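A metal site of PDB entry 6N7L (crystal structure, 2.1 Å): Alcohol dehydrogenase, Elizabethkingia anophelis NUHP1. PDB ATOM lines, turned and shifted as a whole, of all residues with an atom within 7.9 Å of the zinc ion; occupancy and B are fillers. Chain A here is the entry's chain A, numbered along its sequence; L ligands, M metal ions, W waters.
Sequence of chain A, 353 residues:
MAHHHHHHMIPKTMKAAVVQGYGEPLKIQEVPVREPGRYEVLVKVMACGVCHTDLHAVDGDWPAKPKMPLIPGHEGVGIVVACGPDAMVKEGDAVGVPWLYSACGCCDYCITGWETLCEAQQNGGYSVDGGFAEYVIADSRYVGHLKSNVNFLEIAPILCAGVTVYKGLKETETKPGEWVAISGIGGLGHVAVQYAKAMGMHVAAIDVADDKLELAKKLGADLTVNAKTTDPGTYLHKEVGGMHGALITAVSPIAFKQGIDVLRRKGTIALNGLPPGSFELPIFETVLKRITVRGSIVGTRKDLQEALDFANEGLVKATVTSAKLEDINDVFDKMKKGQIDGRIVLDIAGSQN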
ATOM      1  N   GLY A  49       1.262  18.415 -20.796  1.00  0.00           N
ATOM      2  CA  GLY A  49       0.561  17.155 -20.881  1.00  0.00           C
ATOM      3  C   GLY A  49       1.003  16.373 -22.100  1.00  0.00           C
ATOM      4  O   GLY A  49       1.430  16.928 -23.115  1.00  0.00           O
ATOM      5  N   VAL A  50       0.937  15.052 -21.998  1.00  0.00           N
ATOM      6  CA  VAL A  50       1.266  14.182 -23.111  1.00  0.00           C
ATOM      7  C   VAL A  50      -0.037  13.701 -23.705  1.00  0.00           C
ATOM      8  O   VAL A  50      -0.794  12.946 -23.067  1.00  0.00           O
ATOM      9  CB  VAL A  50       2.172  13.031 -22.696  1.00  0.00           C
ATOM     10  CG1 VAL A  50       2.471  12.155 -23.925  1.00  0.00           C
ATOM     11  CG2 VAL A  50       3.476  13.571 -22.078  1.00  0.00           C
ATOM     12  N   CYS A  51      -0.290  14.110 -24.947  1.00  0.00           N
ATOM     13  CA  CYS A  51      -1.513  13.809 -25.681  1.00  0.00           C
ATOM     14  C   CYS A  51      -1.221  12.694 -26.677  1.00  0.00           C
ATOM     15  O   CYS A  51      -0.112  12.602 -27.211  1.00  0.00           O
ATOM     16  CB  CYS A  51      -2.014  15.057 -26.405  1.00  0.00           C
ATOM     17  SG  CYS A  51      -3.549  14.846 -27.385  1.00  0.00           S
ATOM     18  N   HIS A  52      -2.225  11.858 -26.964  1.00  0.00           N
ATOM     19  CA  HIS A  52      -2.008  10.763 -27.905  1.00  0.00           C
ATOM     20  C   HIS A  52      -1.662  11.304 -29.282  1.00  0.00           C
ATOM     21  O   HIS A  52      -0.982  10.633 -30.064  1.00  0.00           O
ATOM     22  CB  HIS A  52      -3.234   9.856 -27.951  1.00  0.00           C
ATOM     23  CG  HIS A  52      -2.970   8.468 -28.449  1.00  0.00           C
ATOM     24  ND1 HIS A  52      -3.126   7.347 -27.652  1.00  0.00           N
ATOM     25  CD2 HIS A  52      -2.570   8.008 -29.664  1.00  0.00           C
ATOM     26  CE1 HIS A  52      -2.824   6.266 -28.352  1.00  0.00           C
ATOM     27  NE2 HIS A  52      -2.490   6.637 -29.576  1.00  0.00           N
ATOM     28  N   THR A  53      -2.091  12.533 -29.569  1.00  0.00           N
ATOM     29  CA  THR A  53      -1.674  13.200 -30.800  1.00  0.00           C
ATOM     30  C   THR A  53      -0.152  13.275 -30.897  1.00  0.00           C
ATOM     31  O   THR A  53       0.403  13.061 -31.967  1.00  0.00           O
ATOM     32  CB  THR A  53      -2.306  14.594 -30.875  1.00  0.00           C
ATOM     33  OG1 THR A  53      -3.705  14.465 -31.160  1.00  0.00           O
ATOM     34  CG2 THR A  53      -1.661  15.421 -31.976  1.00  0.00           C
ATOM     35  N   ASP A  54       0.532  13.551 -29.780  1.00  0.00           N
ATOM     36  CA  ASP A  54       1.991  13.510 -29.769  1.00  0.00           C
ATOM     37  C   ASP A  54       2.522  12.156 -30.238  1.00  0.00           C
ATOM     38  O   ASP A  54       3.576  12.068 -30.870  1.00  0.00           O
ATOM     39  CB  ASP A  54       2.537  13.831 -28.380  1.00  0.00           C
ATOM     40  CG  ASP A  54       2.166  15.227 -27.913  1.00  0.00           C
ATOM     41  OD1 ASP A  54       2.385  16.188 -28.687  1.00  0.00           O
ATOM     42  OD2 ASP A  54       1.663  15.367 -26.784  1.00  0.00           O
ATOM     43  N   TRP A  62      -0.501   9.993 -39.480  1.00  0.00           N
ATOM     44  CA  TRP A  62      -1.483  10.768 -40.226  1.00  0.00           C
ATOM     45  C   TRP A  62      -0.985  11.095 -41.628  1.00  0.00           C
ATOM     46  O   TRP A  62       0.218  11.138 -41.865  1.00  0.00           O
ATOM     47  CB  TRP A  62      -1.812  12.067 -39.489  1.00  0.00           C
ATOM     48  CG  TRP A  62      -2.499  11.848 -38.195  1.00  0.00           C
ATOM     49  CD1 TRP A  62      -3.122  10.711 -37.777  1.00  0.00           C
ATOM     50  CD2 TRP A  62      -2.611  12.792 -37.126  1.00  0.00           C
ATOM     51  NE1 TRP A  62      -3.631  10.899 -36.508  1.00  0.00           N
ATOM     52  CE2 TRP A  62      -3.324  12.170 -36.084  1.00  0.00           C
ATOM     53  CE3 TRP A  62      -2.183  14.116 -36.943  1.00  0.00           C
ATOM     54  CZ2 TRP A  62      -3.626  12.816 -34.890  1.00  0.00           C
ATOM     55  CZ3 TRP A  62      -2.485  14.762 -35.750  1.00  0.00           C
ATOM     56  CH2 TRP A  62      -3.206  14.108 -34.741  1.00  0.00           C
ATOM     57  N   GLY A  73       4.268  18.316 -28.193  1.00  0.00           N
ATOM     58  CA  GLY A  73       3.705  18.914 -26.992  1.00  0.00           C
ATOM     59  C   GLY A  73       2.869  20.146 -27.257  1.00  0.00           C
ATOM     60  O   GLY A  73       3.365  21.195 -27.643  1.00  0.00           O
ATOM     61  N   HIS A  74       1.567  20.017 -27.025  1.00  0.00           N
ATOM     62  CA  HIS A  74       0.650  21.136 -27.167  1.00  0.00           C
ATOM     63  C   HIS A  74      -0.303  21.167 -25.988  1.00  0.00           C
ATOM     64  O   HIS A  74      -1.453  21.583 -26.125  1.00  0.00           O
ATOM     65  CB  HIS A  74      -0.131  21.042 -28.479  1.00  0.00           C
ATOM     66  CG  HIS A  74      -0.798  19.727 -28.668  1.00  0.00           C
ATOM     67  ND1 HIS A  74      -0.225  18.696 -29.366  1.00  0.00           N
ATOM     68  CD2 HIS A  74      -1.979  19.267 -28.197  1.00  0.00           C
ATOM     69  CE1 HIS A  74      -1.032  17.643 -29.339  1.00  0.00           C
ATOM     70  NE2 HIS A  74      -2.105  17.967 -28.643  1.00  0.00           N
ATOM     71  N   GLU A  75       0.142  20.667 -24.849  1.00  0.00           N
ATOM     72  CA  GLU A  75      -0.523  20.885 -23.572  1.00  0.00           C
ATOM     73  C   GLU A  75       0.444  21.558 -22.611  1.00  0.00           C
ATOM     74  O   GLU A  75       0.445  21.305 -21.403  1.00  0.00           O
ATOM     75  CB  GLU A  75      -1.057  19.580 -22.997  1.00  0.00           C
ATOM     76  CG  GLU A  75      -2.254  19.064 -23.776  1.00  0.00           C
ATOM     77  CD  GLU A  75      -2.992  17.897 -23.098  1.00  0.00           C
ATOM     78  OE1 GLU A  75      -2.449  17.322 -22.138  1.00  0.00           O
ATOM     79  OE2 GLU A  75      -4.103  17.537 -23.549  1.00  0.00           O
ATOM     80  N   PRO A  98      -1.585  25.751 -27.018  1.00  0.00           N
ATOM     81  CA  PRO A  98      -2.388  24.591 -27.416  1.00  0.00           C
ATOM     82  C   PRO A  98      -2.156  24.150 -28.854  1.00  0.00           C
ATOM     83  O   PRO A  98      -1.291  24.687 -29.554  1.00  0.00           O
ATOM     84  CB  PRO A  98      -3.824  25.097 -27.236  1.00  0.00           C
ATOM     85  CG  PRO A  98      -3.716  26.541 -27.700  1.00  0.00           C
ATOM     86  CD  PRO A  98      -2.297  27.011 -27.317  1.00  0.00           C
ATOM     87  N   TRP A  99      -2.952  23.163 -29.294  1.00  0.00           N
ATOM     88  CA  TRP A  99      -2.870  22.675 -30.680  1.00  0.00           C
ATOM     89  C   TRP A  99      -3.143  23.785 -31.675  1.00  0.00           C
ATOM     90  O   TRP A  99      -2.411  23.945 -32.662  1.00  0.00           O
ATOM     91  CB  TRP A  99      -3.847  21.519 -30.869  1.00  0.00           C
ATOM     92  CG  TRP A  99      -3.978  21.025 -32.273  1.00  0.00           C
ATOM     93  CD1 TRP A  99      -5.002  21.284 -33.149  1.00  0.00           C
ATOM     94  CD2 TRP A  99      -3.085  20.138 -32.950  1.00  0.00           C
ATOM     95  NE1 TRP A  99      -4.773  20.631 -34.343  1.00  0.00           N
ATOM     96  CE2 TRP A  99      -3.607  19.914 -34.241  1.00  0.00           C
ATOM     97  CE3 TRP A  99      -1.888  19.518 -32.608  1.00  0.00           C
ATOM     98  CZ2 TRP A  99      -2.972  19.103 -35.179  1.00  0.00           C
ATOM     99  CZ3 TRP A  99      -1.252  18.703 -33.537  1.00  0.00           C
ATOM    100  CH2 TRP A  99      -1.799  18.507 -34.812  1.00  0.00           C
ATOM    101  N   GLY A 124       0.673  23.447 -32.618  1.00  0.00           N
ATOM    102  CA  GLY A 124       1.763  23.333 -31.664  1.00  0.00           C
ATOM    103  C   GLY A 124       2.229  21.888 -31.502  1.00  0.00           C
ATOM    104  O   GLY A 124       1.434  20.953 -31.408  1.00  0.00           O
ATOM    105  N   PRO A 157      -3.749  19.319 -18.951  1.00  0.00           N
ATOM    106  CA  PRO A 157      -4.610  18.631 -19.926  1.00  0.00           C
ATOM    107  C   PRO A 157      -5.784  19.453 -20.411  1.00  0.00           C
ATOM    108  O   PRO A 157      -6.362  19.096 -21.449  1.00  0.00           O
ATOM    109  CB  PRO A 157      -5.063  17.372 -19.173  1.00  0.00           C
ATOM    110  CG  PRO A 157      -3.999  17.147 -18.137  1.00  0.00           C
ATOM    111  CD  PRO A 157      -3.640  18.529 -17.702  1.00  0.00           C
ATOM    112  N   LEU A 159      -5.676  22.211 -21.775  1.00  0.00           N
ATOM    113  CA  LEU A 159      -5.224  22.896 -22.983  1.00  0.00           C
ATOM    114  C   LEU A 159      -5.443  22.073 -24.249  1.00  0.00           C
ATOM    115  O   LEU A 159      -5.402  22.639 -25.353  1.00  0.00           O
ATOM    116  CB  LEU A 159      -3.733  23.225 -22.855  1.00  0.00           C
ATOM    117  CG  LEU A 159      -3.385  24.598 -22.290  1.00  0.00           C
ATOM    118  CD1 LEU A 159      -3.828  25.731 -23.233  1.00  0.00           C
ATOM    119  CD2 LEU A 159      -4.030  24.763 -20.939  1.00  0.00           C
ATOM    120  N   CYS A 160      -5.666  20.766 -24.135  1.00  0.00           N
ATOM    121  CA  CYS A 160      -6.074  20.017 -25.316  1.00  0.00           C
ATOM    122  C   CYS A 160      -7.152  18.995 -24.998  1.00  0.00           C
ATOM    123  O   CYS A 160      -8.261  19.077 -25.536  1.00  0.00           O
ATOM    124  CB  CYS A 160      -4.897  19.307 -25.987  1.00  0.00           C
ATOM    125  SG  CYS A 160      -5.404  18.659 -27.611  1.00  0.00           S
ATOM    126  N   ALA A 161      -6.866  18.060 -24.089  1.00  0.00           N
ATOM    127  CA  ALA A 161      -7.870  17.075 -23.693  1.00  0.00           C
ATOM    128  C   ALA A 161      -9.172  17.761 -23.282  1.00  0.00           C
ATOM    129  O   ALA A 161     -10.256  17.386 -23.743  1.00  0.00           O
ATOM    130  CB  ALA A 161      -7.331  16.203 -22.544  1.00  0.00           C
ATOM    131  N   THR A 164     -10.987  20.071 -26.028  1.00  0.00           N
ATOM    132  CA  THR A 164     -11.439  19.219 -27.121  1.00  0.00           C
ATOM    133  C   THR A 164     -12.753  18.531 -26.791  1.00  0.00           C
ATOM    134  O   THR A 164     -13.711  18.582 -27.577  1.00  0.00           O
ATOM    135  CB  THR A 164     -10.391  18.164 -27.457  1.00  0.00           C
ATOM    136  OG1 THR A 164      -9.206  18.789 -27.985  1.00  0.00           O
ATOM    137  CG2 THR A 164     -10.975  17.126 -28.480  1.00  0.00           C
ATOM    138  N   LEU A 188      -8.479  12.150 -23.017  1.00  0.00           N
ATOM    139  CA  LEU A 188      -9.676  12.913 -23.357  1.00  0.00           C
ATOM    140  C   LEU A 188     -10.889  12.395 -22.598  1.00  0.00           C
ATOM    141  O   LEU A 188     -11.644  13.173 -21.999  1.00  0.00           O
ATOM    142  CB  LEU A 188      -9.925  12.821 -24.864  1.00  0.00           C
ATOM    143  CG  LEU A 188      -9.271  13.900 -25.725  1.00  0.00           C
ATOM    144  CD1 LEU A 188      -7.740  13.798 -25.698  1.00  0.00           C
ATOM    145  CD2 LEU A 188      -9.798  13.782 -27.136  1.00  0.00           C
ATOM    146  N   LEU A 274      -8.489  10.059 -33.373  1.00  0.00           N
ATOM    147  CA  LEU A 274      -7.816  10.197 -34.652  1.00  0.00           C
ATOM    148  C   LEU A 274      -6.922   9.000 -35.006  1.00  0.00           C
ATOM    149  O   LEU A 274      -5.782   9.171 -35.442  1.00  0.00           O
ATOM    150  CB  LEU A 274      -7.001  11.489 -34.652  1.00  0.00           C
ATOM    151  CG  LEU A 274      -7.803  12.796 -34.763  1.00  0.00           C
ATOM    152  CD1 LEU A 274      -6.906  14.031 -34.452  1.00  0.00           C
ATOM    153  CD2 LEU A 274      -8.423  12.933 -36.155  1.00  0.00           C
ATOM    154  N   VAL A 298     -10.439  20.138 -31.719  1.00  0.00           N
ATOM    155  CA  VAL A 298     -10.103  20.961 -30.551  1.00  0.00           C
ATOM    156  C   VAL A 298     -11.210  21.983 -30.250  1.00  0.00           C
ATOM    157  O   VAL A 298     -12.389  21.609 -30.213  1.00  0.00           O
ATOM    158  CB  VAL A 298      -8.698  21.604 -30.708  1.00  0.00           C
ATOM    159  CG1 VAL A 298      -7.630  20.475 -30.750  1.00  0.00           C
ATOM    160  CG2 VAL A 298      -8.569  22.499 -31.949  1.00  0.00           C
ATOM    161  N   ARG A 343      -4.134  10.984 -17.633  1.00  0.00           N
ATOM    162  CA  ARG A 343      -3.100  11.717 -18.363  1.00  0.00           C
ATOM    163  C   ARG A 343      -1.762  11.593 -17.643  1.00  0.00           C
ATOM    164  O   ARG A 343      -1.705  11.571 -16.419  1.00  0.00           O
ATOM    165  CB  ARG A 343      -3.461  13.216 -18.479  1.00  0.00           C
ATOM    166  CG  ARG A 343      -4.074  13.656 -19.829  1.00  0.00           C
ATOM    167  CD  ARG A 343      -3.002  13.840 -20.891  1.00  0.00           C
ATOM    168  NE  ARG A 343      -3.484  14.580 -22.048  1.00  0.00           N
ATOM    169  CZ  ARG A 343      -4.046  14.016 -23.106  1.00  0.00           C
ATOM    170  NH1 ARG A 343      -4.183  12.699 -23.175  1.00  0.00           N
ATOM    171  NH2 ARG A 343      -4.447  14.775 -24.117  1.00  0.00           N
HETATM  172  P1  LIG L   1      -5.323   7.857 -24.691  1.00  0.00           P
HETATM  173  O1  LIG L   1      -5.028   8.519 -23.404  1.00  0.00           O
HETATM  174  O2  LIG L   1      -4.264   6.891 -25.169  1.00  0.00           O
HETATM  175  O3  LIG L   1      -6.691   7.046 -24.564  1.00  0.00           O
HETATM  176  C1  LIG L   1      -7.260   6.215 -25.594  1.00  0.00           C
HETATM  177  C2  LIG L   1      -8.340   5.418 -24.903  1.00  0.00           C
HETATM  178  O4  LIG L   1      -9.109   4.662 -25.868  1.00  0.00           O
HETATM  179  C3  LIG L   1      -7.848   4.413 -23.852  1.00  0.00           C
HETATM  180  O5  LIG L   1      -8.563   4.592 -22.636  1.00  0.00           O
HETATM  181  C4  LIG L   1      -8.174   3.058 -24.491  1.00  0.00           C
HETATM  182  O6  LIG L   1      -8.435   2.051 -23.521  1.00  0.00           O
HETATM  183  C5  LIG L   1      -9.430   3.439 -25.255  1.00  0.00           C
HETATM  184  N1  LIG L   1      -9.842   2.493 -26.273  1.00  0.00           N
HETATM  185  C6  LIG L   1      -9.048   1.738 -27.109  1.00  0.00           C
HETATM  186  N2  LIG L   1      -9.718   0.927 -27.895  1.00  0.00           N
HETATM  187  C7  LIG L   1     -11.048   1.164 -27.557  1.00  0.00           C
HETATM  188  C8  LIG L   1     -12.252   0.622 -28.041  1.00  0.00           C
HETATM  189  N3  LIG L   1     -12.324  -0.325 -28.980  1.00  0.00           N
HETATM  190  N4  LIG L   1     -13.400   1.097 -27.501  1.00  0.00           N
HETATM  191  C9  LIG L   1     -13.334   2.035 -26.554  1.00  0.00           C
HETATM  192  N5  LIG L   1     -12.254   2.608 -26.013  1.00  0.00           N
HETATM  193  C10 LIG L   1     -11.132   2.122 -26.575  1.00  0.00           C
HETATM  194  O7  LIG L   1      -5.448   8.953 -25.839  1.00  0.00           O
HETATM  195  P2  LIG L   1      -5.979  10.456 -25.792  1.00  0.00           P
HETATM  196  O8  LIG L   1      -4.865  11.377 -25.480  1.00  0.00           O
HETATM  197  O9  LIG L   1      -7.212  10.495 -24.972  1.00  0.00           O
HETATM  198  O10 LIG L   1      -6.322  10.677 -27.332  1.00  0.00           O
HETATM  199  C11 LIG L   1      -7.348   9.892 -27.955  1.00  0.00           C
HETATM  200  C12 LIG L   1      -7.421  10.215 -29.428  1.00  0.00           C
HETATM  201  O11 LIG L   1      -7.979  11.538 -29.622  1.00  0.00           O
HETATM  202  C13 LIG L   1      -6.097  10.184 -30.196  1.00  0.00           C
HETATM  203  O12 LIG L   1      -6.369   9.688 -31.509  1.00  0.00           O
HETATM  204  C14 LIG L   1      -5.731  11.660 -30.281  1.00  0.00           C
HETATM  205  O13 LIG L   1      -4.876  11.973 -31.373  1.00  0.00           O
HETATM  206  C15 LIG L   1      -7.123  12.256 -30.477  1.00  0.00           C
HETATM  207  N6  LIG L   1      -7.240  13.743 -30.130  1.00  0.00           N
HETATM  208  C16 LIG L   1      -8.024  14.446 -30.952  1.00  0.00           C
HETATM  209  C17 LIG L   1      -8.284  15.776 -30.707  1.00  0.00           C
HETATM  210  C18 LIG L   1      -9.315  16.541 -31.513  1.00  0.00           C
HETATM  211  O14 LIG L   1      -9.370  17.770 -31.411  1.00  0.00           O
HETATM  212  N7  LIG L   1     -10.067  15.858 -32.375  1.00  0.00           N
HETATM  213  C19 LIG L   1      -7.679  16.373 -29.590  1.00  0.00           C
HETATM  214  C20 LIG L   1      -6.880  15.615 -28.749  1.00  0.00           C
HETATM  215  C21 LIG L   1      -6.665  14.285 -29.040  1.00  0.00           C
HETATM  216 ZN    ZN M   1      -3.915  16.988 -28.348  1.00  0.00          ZN
HETATM  217  O   HOH W   1      -4.564  16.928 -30.445  1.00  0.00           O
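The backbone NH (N) of Leu 274 is in hydrogen-bond range of an oxygen (O12) of the ligand, at 2.8 Å.
The side-chain hydroxyl (OG1) of Thr 53 sits at hydrogen-bond distance from an oxygen (O13) of the ligand, 2.8 Å away.
A ring nitrogen (ND1) of His 52 lies within hydrogen-bond range of an oxygen (O2) of the ligand (2.8 Å).
The backbone NH (N) of Val 298 sits at hydrogen-bond distance from an oxygen (O14) of the ligand (2.6 Å).
N of His 52 lies within hydrogen-bond range of O8 of the ligand (3.1 Å).
The guanidinium group of Arg 343 is in salt-bridge range of an oxygen (O8) of the ligand, at 2.7 Å.
The backbone NH of Thr 53 sits at hydrogen-bond distance from an oxygen (O13) of the ligand, 3.4 Å away.
The backbone NH (N) of Leu 188 lies within hydrogen-bond range of an oxygen (O9) of the ligand (2.9 Å).
The side-chain sulfur (SG) of Cys 51 sits close to the guanidinium group (NH2) of Arg 343 (3.4 Å).
The side-chain sulfur (SG) of Cys 51 lies close to the backbone NH (N) of Thr 53 (3.5 Å).
OG1 of Thr 164 is in hydrogen-bond range of O of Cys 160 (2.6 Å).
The backbone NH of Cys 51 is in hydrogen-bond range of the side-chain carboxylate of Asp 54 (3.0 Å).
A ring nitrogen (ND1) of His 74 sits close to the backbone carbonyl oxygen (O) of Gly 124, at 3.5 Å.
Thr 53 touches the zinc ion (OG1 to ZN, 3.8 Å).
Of the 22 residues printed, 4 come within 4 Å of the zinc ion.
The zinc ion is bound by NE2 of His 74, water W1, SG of Cys 160 and SG of Cys 51.
The zinc ion has four donor atoms within binding distance.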
